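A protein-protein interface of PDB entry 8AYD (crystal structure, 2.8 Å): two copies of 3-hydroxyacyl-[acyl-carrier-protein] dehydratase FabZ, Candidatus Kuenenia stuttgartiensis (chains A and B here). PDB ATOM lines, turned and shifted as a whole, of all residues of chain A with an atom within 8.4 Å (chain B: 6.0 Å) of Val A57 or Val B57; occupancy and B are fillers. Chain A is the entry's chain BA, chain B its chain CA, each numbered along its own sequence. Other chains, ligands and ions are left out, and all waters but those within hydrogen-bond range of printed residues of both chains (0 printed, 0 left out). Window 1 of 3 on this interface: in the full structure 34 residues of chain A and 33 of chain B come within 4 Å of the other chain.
The side-chain amide nitrogen (NE2) of Gln A65 is in hydrogen-bond range of the side-chain carboxylate (OE2) of Glu A61, 3.5 Å away.
The side-chain amide nitrogen of Gln A65 sits at hydrogen-bond distance from the backbone carbonyl oxygen of Phe A16.
Among the printed residues, pairs that only touch across the chains: Val A57 with Val B57, Leu A87 with Phe B95, Val A57 with Glu B61, Phe A95 with Leu B87, Phe A16 with Pro B55, Glu A61 with Val B57, Val A43 with Phe B16, Ile A60 with Val B57, Pro A55 with Phe B16, Val A57 with Leu B87, Val A57 with Ile B60, Val A57 with Phe B16, His A47 with Phe B16, Leu A58 with Phe B16 and Phe A16 with Leu B58.
Hydrophobic or aromatic side chains of chain B within 4 Å of the printed part of chain A: Phe B16, Pro B55, Val B57, Leu B58, Ile B60, Leu B87 and Phe B95.
Along chain B the printed residues that touch a printed residue of chain A span positions 16 to 95.
Of the 20 printed residues of chain A, 10 touch a printed residue of chain B.
Printed residues of chain A that touch a printed residue of chain B: Phe A16, Val A43, His A47, Pro A55, Val A57, Leu A58, Ile A60, Glu A61, Leu A87 and Phe A95.
Hydrophobic or aromatic side chains of chain A within 4 Å of the printed part of chain B: Phe A16, Val A43, His A47, Pro A55, Val A57, Leu A58, Ile A60, Leu A87 and Phe A95.
Val A57 touches its own counterpart, Val B57.
Val A57 touches Ile B60, and with the chains exchanged Ile A60 touches Val B57.
Val A57 touches Glu B61, and with the chains exchanged Glu A61 touches Val B57.
Val A57 touches Leu B87, but with the chains exchanged Leu A87 does not touch Val B57 (4.004 Å).
11 positions are printed for both chains.
Val A57 touches five residues of chain B.
Of the printed residues of chain A, Val B57 touches Val A57, Ile A60 and Glu A61.
No residue of chain A comes within 4 Å of Gly B56.
Of the printed residues of chain A, Glu B61 touches Val A57 (3.5 Å).
Of the printed residues of chain A, Leu B87 touches Val A57 and Phe A95.
Ala A64 touches none of the printed residues of chain B.
Gly A56 touches none of the printed residues of chain B.
The nearest residue of chain B that does not touch Val A57 is Leu B58 (4.7 Å).
The nearest printed residue of chain A that does not touch Val B57 is Leu A87 (4.004 Å).
The nearest printed residue of chain A that does not touch Leu B58 is Leu A58 (4.2 Å).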
ATOM      1  N   PHE A  16       9.585  -6.416   5.410  1.00  0.00           N
ATOM      2  CA  PHE A  16       9.272  -7.807   5.680  1.00  0.00           C
ATOM      3  C   PHE A  16      10.173  -8.366   6.776  1.00  0.00           C
ATOM      4  O   PHE A  16      10.510  -9.555   6.767  1.00  0.00           O
ATOM      5  CB  PHE A  16       9.371  -8.610   4.385  1.00  0.00           C
ATOM      6  CG  PHE A  16       8.425  -9.762   4.318  1.00  0.00           C
ATOM      7  CD1 PHE A  16       7.068  -9.527   4.158  1.00  0.00           C
ATOM      8  CD2 PHE A  16       8.873 -11.066   4.370  1.00  0.00           C
ATOM      9  CE1 PHE A  16       6.172 -10.569   4.080  1.00  0.00           C
ATOM     10  CE2 PHE A  16       7.980 -12.114   4.286  1.00  0.00           C
ATOM     11  CZ  PHE A  16       6.628 -11.865   4.145  1.00  0.00           C
ATOM     12  N   PHE A  18      10.508  -9.427  10.614  1.00  0.00           N
ATOM     13  CA  PHE A  18       9.613  -9.825  11.694  1.00  0.00           C
ATOM     14  C   PHE A  18      10.374 -10.393  12.886  1.00  0.00           C
ATOM     15  O   PHE A  18       9.797 -11.135  13.689  1.00  0.00           O
ATOM     16  CB  PHE A  18       8.574 -10.822  11.181  1.00  0.00           C
ATOM     17  CG  PHE A  18       7.653 -10.243  10.146  1.00  0.00           C
ATOM     18  CD1 PHE A  18       6.579  -9.451  10.518  1.00  0.00           C
ATOM     19  CD2 PHE A  18       7.873 -10.474   8.798  1.00  0.00           C
ATOM     20  CE1 PHE A  18       5.736  -8.909   9.566  1.00  0.00           C
ATOM     21  CE2 PHE A  18       7.033  -9.937   7.841  1.00  0.00           C
ATOM     22  CZ  PHE A  18       5.963  -9.152   8.226  1.00  0.00           C
ATOM     23  N   VAL A  43       1.575  -3.115   8.089  1.00  0.00           N
ATOM     24  CA  VAL A  43       0.514  -4.068   7.785  1.00  0.00           C
ATOM     25  C   VAL A  43      -0.805  -3.703   8.463  1.00  0.00           C
ATOM     26  O   VAL A  43      -1.875  -4.082   7.969  1.00  0.00           O
ATOM     27  CB  VAL A  43       0.958  -5.490   8.178  1.00  0.00           C
ATOM     28  CG1 VAL A  43       1.114  -5.609   9.688  1.00  0.00           C
ATOM     29  CG2 VAL A  43      -0.015  -6.533   7.637  1.00  0.00           C
ATOM     30  N   HIS A  47      -4.774  -4.405   7.668  1.00  0.00           N
ATOM     31  CA  HIS A  47      -5.231  -5.626   8.336  1.00  0.00           C
ATOM     32  C   HIS A  47      -5.308  -5.383   9.843  1.00  0.00           C
ATOM     33  O   HIS A  47      -4.354  -5.670  10.570  1.00  0.00           O
ATOM     34  CB  HIS A  47      -4.294  -6.789   8.009  1.00  0.00           C
ATOM     35  CG  HIS A  47      -4.774  -8.116   8.508  1.00  0.00           C
ATOM     36  ND1 HIS A  47      -4.566  -8.546   9.801  1.00  0.00           N
ATOM     37  CD2 HIS A  47      -5.429  -9.121   7.879  1.00  0.00           C
ATOM     38  CE1 HIS A  47      -5.085  -9.751   9.952  1.00  0.00           C
ATOM     39  NE2 HIS A  47      -5.615 -10.124   8.801  1.00  0.00           N
ATOM     40  N   MET A  54      -2.540  -8.800  14.137  1.00  0.00           N
ATOM     41  CA  MET A  54      -1.378  -9.353  13.454  1.00  0.00           C
ATOM     42  C   MET A  54      -1.828 -10.519  12.583  1.00  0.00           C
ATOM     43  O   MET A  54      -2.402 -11.483  13.108  1.00  0.00           O
ATOM     44  CB  MET A  54      -0.340  -9.808  14.472  1.00  0.00           C
ATOM     45  CG  MET A  54       1.006 -10.225  13.906  1.00  0.00           C
ATOM     46  SD  MET A  54       1.951  -8.842  13.240  1.00  0.00           S
ATOM     47  CE  MET A  54       3.114  -9.702  12.188  1.00  0.00           C
ATOM     48  N   PRO A  55      -1.619 -10.471  11.266  1.00  0.00           N
ATOM     49  CA  PRO A  55      -2.066 -11.577  10.411  1.00  0.00           C
ATOM     50  C   PRO A  55      -1.395 -12.883  10.802  1.00  0.00           C
ATOM     51  O   PRO A  55      -0.219 -12.915  11.169  1.00  0.00           O
ATOM     52  CB  PRO A  55      -1.649 -11.129   9.005  1.00  0.00           C
ATOM     53  CG  PRO A  55      -1.551  -9.644   9.096  1.00  0.00           C
ATOM     54  CD  PRO A  55      -1.047  -9.365  10.482  1.00  0.00           C
ATOM     55  N   GLY A  56      -2.165 -13.970  10.729  1.00  0.00           N
ATOM     56  CA  GLY A  56      -1.626 -15.265  11.102  1.00  0.00           C
ATOM     57  C   GLY A  56      -0.473 -15.698  10.219  1.00  0.00           C
ATOM     58  O   GLY A  56       0.508 -16.271  10.699  1.00  0.00           O
ATOM     59  N   VAL A  57      -0.563 -15.411   8.918  1.00  0.00           N
ATOM     60  CA  VAL A  57       0.492 -15.818   7.996  1.00  0.00           C
ATOM     61  C   VAL A  57       1.813 -15.150   8.349  1.00  0.00           C
ATOM     62  O   VAL A  57       2.883 -15.753   8.193  1.00  0.00           O
ATOM     63  CB  VAL A  57       0.077 -15.514   6.543  1.00  0.00           C
ATOM     64  CG1 VAL A  57      -1.164 -16.307   6.170  1.00  0.00           C
ATOM     65  CG2 VAL A  57      -0.162 -14.025   6.361  1.00  0.00           C
ATOM     66  N   LEU A  58       1.772 -13.909   8.836  1.00  0.00           N
ATOM     67  CA  LEU A  58       3.001 -13.218   9.192  1.00  0.00           C
ATOM     68  C   LEU A  58       3.592 -13.731  10.497  1.00  0.00           C
ATOM     69  O   LEU A  58       4.778 -13.502  10.759  1.00  0.00           O
ATOM     70  CB  LEU A  58       2.757 -11.711   9.277  1.00  0.00           C
ATOM     71  CG  LEU A  58       2.292 -11.059   7.973  1.00  0.00           C
ATOM     72  CD1 LEU A  58       2.086  -9.561   8.157  1.00  0.00           C
ATOM     73  CD2 LEU A  58       3.249 -11.353   6.824  1.00  0.00           C
ATOM     74  N   ILE A  59       2.793 -14.415  11.319  1.00  0.00           N
ATOM     75  CA  ILE A  59       3.350 -15.122  12.467  1.00  0.00           C
ATOM     76  C   ILE A  59       4.154 -16.327  11.997  1.00  0.00           C
ATOM     77  O   ILE A  59       5.186 -16.672  12.587  1.00  0.00           O
ATOM     78  CB  ILE A  59       2.228 -15.525  13.442  1.00  0.00           C
ATOM     79  CG1 ILE A  59       1.508 -14.284  13.969  1.00  0.00           C
ATOM     80  CG2 ILE A  59       2.789 -16.334  14.601  1.00  0.00           C
ATOM     81  CD1 ILE A  59       0.237 -14.595  14.730  1.00  0.00           C
ATOM     82  N   ILE A  60       3.704 -16.977  10.919  1.00  0.00           N
ATOM     83  CA  ILE A  60       4.469 -18.076  10.334  1.00  0.00           C
ATOM     84  C   ILE A  60       5.794 -17.565   9.786  1.00  0.00           C
ATOM     85  O   ILE A  60       6.844 -18.196   9.965  1.00  0.00           O
ATOM     86  CB  ILE A  60       3.646 -18.783   9.242  1.00  0.00           C
ATOM     87  CG1 ILE A  60       2.387 -19.415   9.834  1.00  0.00           C
ATOM     88  CG2 ILE A  60       4.482 -19.839   8.538  1.00  0.00           C
ATOM     89  CD1 ILE A  60       1.422 -19.925   8.785  1.00  0.00           C
ATOM     90  N   GLU A  61       5.769 -16.418   9.103  1.00  0.00           N
ATOM     91  CA  GLU A  61       7.007 -15.830   8.602  1.00  0.00           C
ATOM     92  C   GLU A  61       7.935 -15.453   9.749  1.00  0.00           C
ATOM     93  O   GLU A  61       9.160 -15.573   9.633  1.00  0.00           O
ATOM     94  CB  GLU A  61       6.696 -14.608   7.740  1.00  0.00           C
ATOM     95  CG  GLU A  61       7.918 -13.973   7.101  1.00  0.00           C
ATOM     96  CD  GLU A  61       8.550 -14.854   6.037  1.00  0.00           C
ATOM     97  OE1 GLU A  61       7.831 -15.687   5.446  1.00  0.00           O
ATOM     98  OE2 GLU A  61       9.764 -14.703   5.784  1.00  0.00           O
ATOM     99  N   ALA A  62       7.365 -14.995  10.866  1.00  0.00           N
ATOM    100  CA  ALA A  62       8.175 -14.723  12.049  1.00  0.00           C
ATOM    101  C   ALA A  62       8.795 -16.004  12.591  1.00  0.00           C
ATOM    102  O   ALA A  62       9.947 -16.003  13.039  1.00  0.00           O
ATOM    103  CB  ALA A  62       7.326 -14.035  13.117  1.00  0.00           C
ATOM    104  N   MET A  63       8.042 -17.108  12.562  1.00  0.00           N
ATOM    105  CA  MET A  63       8.625 -18.408  12.876  1.00  0.00           C
ATOM    106  C   MET A  63       9.739 -18.750  11.897  1.00  0.00           C
ATOM    107  O   MET A  63      10.780 -19.290  12.287  1.00  0.00           O
ATOM    108  CB  MET A  63       7.552 -19.495  12.835  1.00  0.00           C
ATOM    109  CG  MET A  63       6.454 -19.388  13.875  1.00  0.00           C
ATOM    110  SD  MET A  63       5.276 -20.739  13.659  1.00  0.00           S
ATOM    111  CE  MET A  63       4.018 -20.321  14.861  1.00  0.00           C
ATOM    112  N   ALA A  64       9.531 -18.443  10.614  1.00  0.00           N
ATOM    113  CA  ALA A  64      10.505 -18.798   9.588  1.00  0.00           C
ATOM    114  C   ALA A  64      11.777 -17.972   9.721  1.00  0.00           C
ATOM    115  O   ALA A  64      12.888 -18.509   9.650  1.00  0.00           O
ATOM    116  CB  ALA A  64       9.888 -18.621   8.200  1.00  0.00           C
ATOM    117  N   GLN A  65      11.634 -16.658   9.915  1.00  0.00           N
ATOM    118  CA  GLN A  65      12.807 -15.797  10.020  1.00  0.00           C
ATOM    119  C   GLN A  65      13.612 -16.089  11.279  1.00  0.00           C
ATOM    120  O   GLN A  65      14.832 -15.885  11.293  1.00  0.00           O
ATOM    121  CB  GLN A  65      12.387 -14.328   9.989  1.00  0.00           C
ATOM    122  CG  GLN A  65      11.799 -13.875   8.664  1.00  0.00           C
ATOM    123  CD  GLN A  65      11.400 -12.413   8.676  1.00  0.00           C
ATOM    124  OE1 GLN A  65      11.515 -11.735   9.698  1.00  0.00           O
ATOM    125  NE2 GLN A  65      10.927 -11.917   7.538  1.00  0.00           N
ATOM    126  N   LEU A  87      10.229 -21.073   2.233  1.00  0.00           N
ATOM    127  CA  LEU A  87       9.321 -21.990   2.906  1.00  0.00           C
ATOM    128  C   LEU A  87       8.787 -23.014   1.911  1.00  0.00           C
ATOM    129  O   LEU A  87       8.311 -22.651   0.831  1.00  0.00           O
ATOM    130  CB  LEU A  87       8.177 -21.208   3.548  1.00  0.00           C
ATOM    131  CG  LEU A  87       7.224 -21.924   4.503  1.00  0.00           C
ATOM    132  CD1 LEU A  87       7.972 -22.380   5.748  1.00  0.00           C
ATOM    133  CD2 LEU A  87       6.071 -21.004   4.873  1.00  0.00           C
ATOM    134  N   VAL A  90       4.220 -26.422   5.443  1.00  0.00           N
ATOM    135  CA  VAL A  90       3.697 -26.045   6.753  1.00  0.00           C
ATOM    136  C   VAL A  90       2.660 -27.084   7.156  1.00  0.00           C
ATOM    137  O   VAL A  90       1.682 -27.301   6.430  1.00  0.00           O
ATOM    138  CB  VAL A  90       3.068 -24.640   6.758  1.00  0.00           C
ATOM    139  CG1 VAL A  90       2.466 -24.334   8.122  1.00  0.00           C
ATOM    140  CG2 VAL A  90       4.092 -23.584   6.377  1.00  0.00           C
ATOM    141  N   PHE A  95      -3.461 -21.633  15.327  1.00  0.00           N
ATOM    142  CA  PHE A  95      -3.431 -20.279  15.870  1.00  0.00           C
ATOM    143  C   PHE A  95      -4.676 -20.124  16.730  1.00  0.00           C
ATOM    144  O   PHE A  95      -5.772 -20.498  16.304  1.00  0.00           O
ATOM    145  CB  PHE A  95      -3.413 -19.141  14.815  1.00  0.00           C
ATOM    146  CG  PHE A  95      -2.501 -19.362  13.606  1.00  0.00           C
ATOM    147  CD1 PHE A  95      -2.223 -20.621  13.095  1.00  0.00           C
ATOM    148  CD2 PHE A  95      -1.829 -18.288  13.056  1.00  0.00           C
ATOM    149  CE1 PHE A  95      -1.397 -20.795  12.015  1.00  0.00           C
ATOM    150  CE2 PHE A  95      -0.975 -18.466  11.986  1.00  0.00           C
ATOM    151  CZ  PHE A  95      -0.764 -19.719  11.467  1.00  0.00           C
ATOM    152  N   LEU A 137       7.599 -26.323  10.460  1.00  0.00           N
ATOM    153  CA  LEU A 137       8.031 -25.717   9.211  1.00  0.00           C
ATOM    154  C   LEU A 137       9.161 -26.525   8.586  1.00  0.00           C
ATOM    155  O   LEU A 137      10.012 -27.079   9.288  1.00  0.00           O
ATOM    156  CB  LEU A 137       8.502 -24.280   9.447  1.00  0.00           C
ATOM    157  CG  LEU A 137       7.531 -23.305  10.116  1.00  0.00           C
ATOM    158  CD1 LEU A 137       8.194 -21.947  10.295  1.00  0.00           C
ATOM    159  CD2 LEU A 137       6.221 -23.185   9.356  1.00  0.00           C
ATOM    160  N   PHE B  16      -2.315  -5.200   2.237  1.00  0.00           N
ATOM    161  CA  PHE B  16      -2.506  -6.605   2.523  1.00  0.00           C
ATOM    162  C   PHE B  16      -3.718  -7.136   1.770  1.00  0.00           C
ATOM    163  O   PHE B  16      -4.491  -7.946   2.286  1.00  0.00           O
ATOM    164  CB  PHE B  16      -2.623  -6.806   4.029  1.00  0.00           C
ATOM    165  CG  PHE B  16      -2.076  -8.109   4.507  1.00  0.00           C
ATOM    166  CD1 PHE B  16      -0.704  -8.306   4.535  1.00  0.00           C
ATOM    167  CD2 PHE B  16      -2.904  -9.117   4.955  1.00  0.00           C
ATOM    168  CE1 PHE B  16      -0.167  -9.491   4.981  1.00  0.00           C
ATOM    169  CE2 PHE B  16      -2.370 -10.305   5.407  1.00  0.00           C
ATOM    170  CZ  PHE B  16      -1.000 -10.495   5.417  1.00  0.00           C
ATOM    171  N   PRO B  55       6.400 -14.172  -1.062  1.00  0.00           N
ATOM    172  CA  PRO B  55       6.535 -15.016   0.131  1.00  0.00           C
ATOM    173  C   PRO B  55       5.444 -16.075   0.189  1.00  0.00           C
ATOM    174  O   PRO B  55       4.294 -15.833  -0.185  1.00  0.00           O
ATOM    175  CB  PRO B  55       6.412 -14.017   1.288  1.00  0.00           C
ATOM    176  CG  PRO B  55       6.808 -12.706   0.694  1.00  0.00           C
ATOM    177  CD  PRO B  55       6.302 -12.743  -0.718  1.00  0.00           C
ATOM    178  N   GLY B  56       5.822 -17.266   0.661  1.00  0.00           N
ATOM    179  CA  GLY B  56       4.866 -18.355   0.751  1.00  0.00           C
ATOM    180  C   GLY B  56       3.730 -18.076   1.714  1.00  0.00           C
ATOM    181  O   GLY B  56       2.604 -18.532   1.498  1.00  0.00           O
ATOM    182  N   VAL B  57       4.003 -17.327   2.784  1.00  0.00           N
ATOM    183  CA  VAL B  57       2.950 -17.004   3.741  1.00  0.00           C
ATOM    184  C   VAL B  57       1.927 -16.062   3.121  1.00  0.00           C
ATOM    185  O   VAL B  57       0.736 -16.129   3.449  1.00  0.00           O
ATOM    186  CB  VAL B  57       3.558 -16.417   5.030  1.00  0.00           C
ATOM    187  CG1 VAL B  57       4.436 -17.448   5.716  1.00  0.00           C
ATOM    188  CG2 VAL B  57       4.356 -15.156   4.726  1.00  0.00           C
ATOM    189  N   LEU B  58       2.356 -15.179   2.219  1.00  0.00           N
ATOM    190  CA  LEU B  58       1.409 -14.290   1.559  1.00  0.00           C
ATOM    191  C   LEU B  58       0.599 -15.020   0.498  1.00  0.00           C
ATOM    192  O   LEU B  58      -0.527 -14.610   0.194  1.00  0.00           O
ATOM    193  CB  LEU B  58       2.141 -13.100   0.942  1.00  0.00           C
ATOM    194  CG  LEU B  58       2.834 -12.160   1.928  1.00  0.00           C
ATOM    195  CD1 LEU B  58       3.557 -11.057   1.179  1.00  0.00           C
ATOM    196  CD2 LEU B  58       1.842 -11.585   2.922  1.00  0.00           C
ATOM    197  N   ILE B  59       1.150 -16.094  -0.074  1.00  0.00           N
ATOM    198  CA  ILE B  59       0.359 -16.948  -0.954  1.00  0.00           C
ATOM    199  C   ILE B  59      -0.762 -17.613  -0.168  1.00  0.00           C
ATOM    200  O   ILE B  59      -1.840 -17.886  -0.712  1.00  0.00           O
ATOM    201  CB  ILE B  59       1.272 -17.981  -1.649  1.00  0.00           C
ATOM    202  CG1 ILE B  59       2.312 -17.268  -2.517  1.00  0.00           C
ATOM    203  CG2 ILE B  59       0.459 -18.945  -2.501  1.00  0.00           C
ATOM    204  CD1 ILE B  59       3.401 -18.180  -3.040  1.00  0.00           C
ATOM    205  N   ILE B  60      -0.540 -17.864   1.125  1.00  0.00           N
ATOM    206  CA  ILE B  60      -1.591 -18.423   1.968  1.00  0.00           C
ATOM    207  C   ILE B  60      -2.725 -17.417   2.147  1.00  0.00           C
ATOM    208  O   ILE B  60      -3.902 -17.795   2.213  1.00  0.00           O
ATOM    209  CB  ILE B  60      -1.007 -18.872   3.321  1.00  0.00           C
ATOM    210  CG1 ILE B  60       0.042 -19.966   3.114  1.00  0.00           C
ATOM    211  CG2 ILE B  60      -2.105 -19.376   4.245  1.00  0.00           C
ATOM    212  CD1 ILE B  60       0.837 -20.290   4.362  1.00  0.00           C
ATOM    213  N   GLU B  61      -2.394 -16.124   2.225  1.00  0.00           N
ATOM    214  CA  GLU B  61      -3.430 -15.095   2.286  1.00  0.00           C
ATOM    215  C   GLU B  61      -4.305 -15.103   1.040  1.00  0.00           C
ATOM    216  O   GLU B  61      -5.535 -15.021   1.135  1.00  0.00           O
ATOM    217  CB  GLU B  61      -2.806 -13.717   2.490  1.00  0.00           C
ATOM    218  CG  GLU B  61      -2.542 -13.388   3.931  1.00  0.00           C
ATOM    219  CD  GLU B  61      -3.831 -13.127   4.688  1.00  0.00           C
ATOM    220  OE1 GLU B  61      -4.788 -12.617   4.067  1.00  0.00           O
ATOM    221  OE2 GLU B  61      -3.891 -13.425   5.900  1.00  0.00           O
ATOM    222  N   ALA B  62      -3.686 -15.180  -0.141  1.00  0.00           N
ATOM    223  CA  ALA B  62      -4.465 -15.271  -1.371  1.00  0.00           C
ATOM    224  C   ALA B  62      -5.432 -16.446  -1.315  1.00  0.00           C
ATOM    225  O   ALA B  62      -6.550 -16.369  -1.841  1.00  0.00           O
ATOM    226  CB  ALA B  62      -3.535 -15.393  -2.577  1.00  0.00           C
ATOM    227  N   LEU B  87      -7.542 -16.833  10.690  1.00  0.00           N
ATOM    228  CA  LEU B  87      -6.897 -18.065  10.254  1.00  0.00           C
ATOM    229  C   LEU B  87      -6.570 -18.924  11.471  1.00  0.00           C
ATOM    230  O   LEU B  87      -5.871 -18.477  12.386  1.00  0.00           O
ATOM    231  CB  LEU B  87      -5.639 -17.732   9.456  1.00  0.00           C
ATOM    232  CG  LEU B  87      -4.942 -18.846   8.680  1.00  0.00           C
ATOM    233  CD1 LEU B  87      -5.872 -19.391   7.609  1.00  0.00           C
ATOM    234  CD2 LEU B  87      -3.657 -18.326   8.060  1.00  0.00           C
ATOM    235  N   PHE B  95       4.618 -25.660  -0.827  1.00  0.00           N
ATOM    236  CA  PHE B  95       4.981 -24.588  -1.750  1.00  0.00           C
ATOM    237  C   PHE B  95       6.011 -25.169  -2.714  1.00  0.00           C
ATOM    238  O   PHE B  95       7.211 -25.180  -2.419  1.00  0.00           O
ATOM    239  CB  PHE B  95       5.526 -23.380  -0.998  1.00  0.00           C
ATOM    240  CG  PHE B  95       4.590 -22.855   0.050  1.00  0.00           C
ATOM    241  CD1 PHE B  95       3.480 -22.104  -0.297  1.00  0.00           C
ATOM    242  CD2 PHE B  95       4.827 -23.114   1.390  1.00  0.00           C
ATOM    243  CE1 PHE B  95       2.620 -21.627   0.675  1.00  0.00           C
ATOM    244  CE2 PHE B  95       3.974 -22.639   2.364  1.00  0.00           C
ATOM    245  CZ  PHE B  95       2.869 -21.895   2.007  1.00  0.00           C
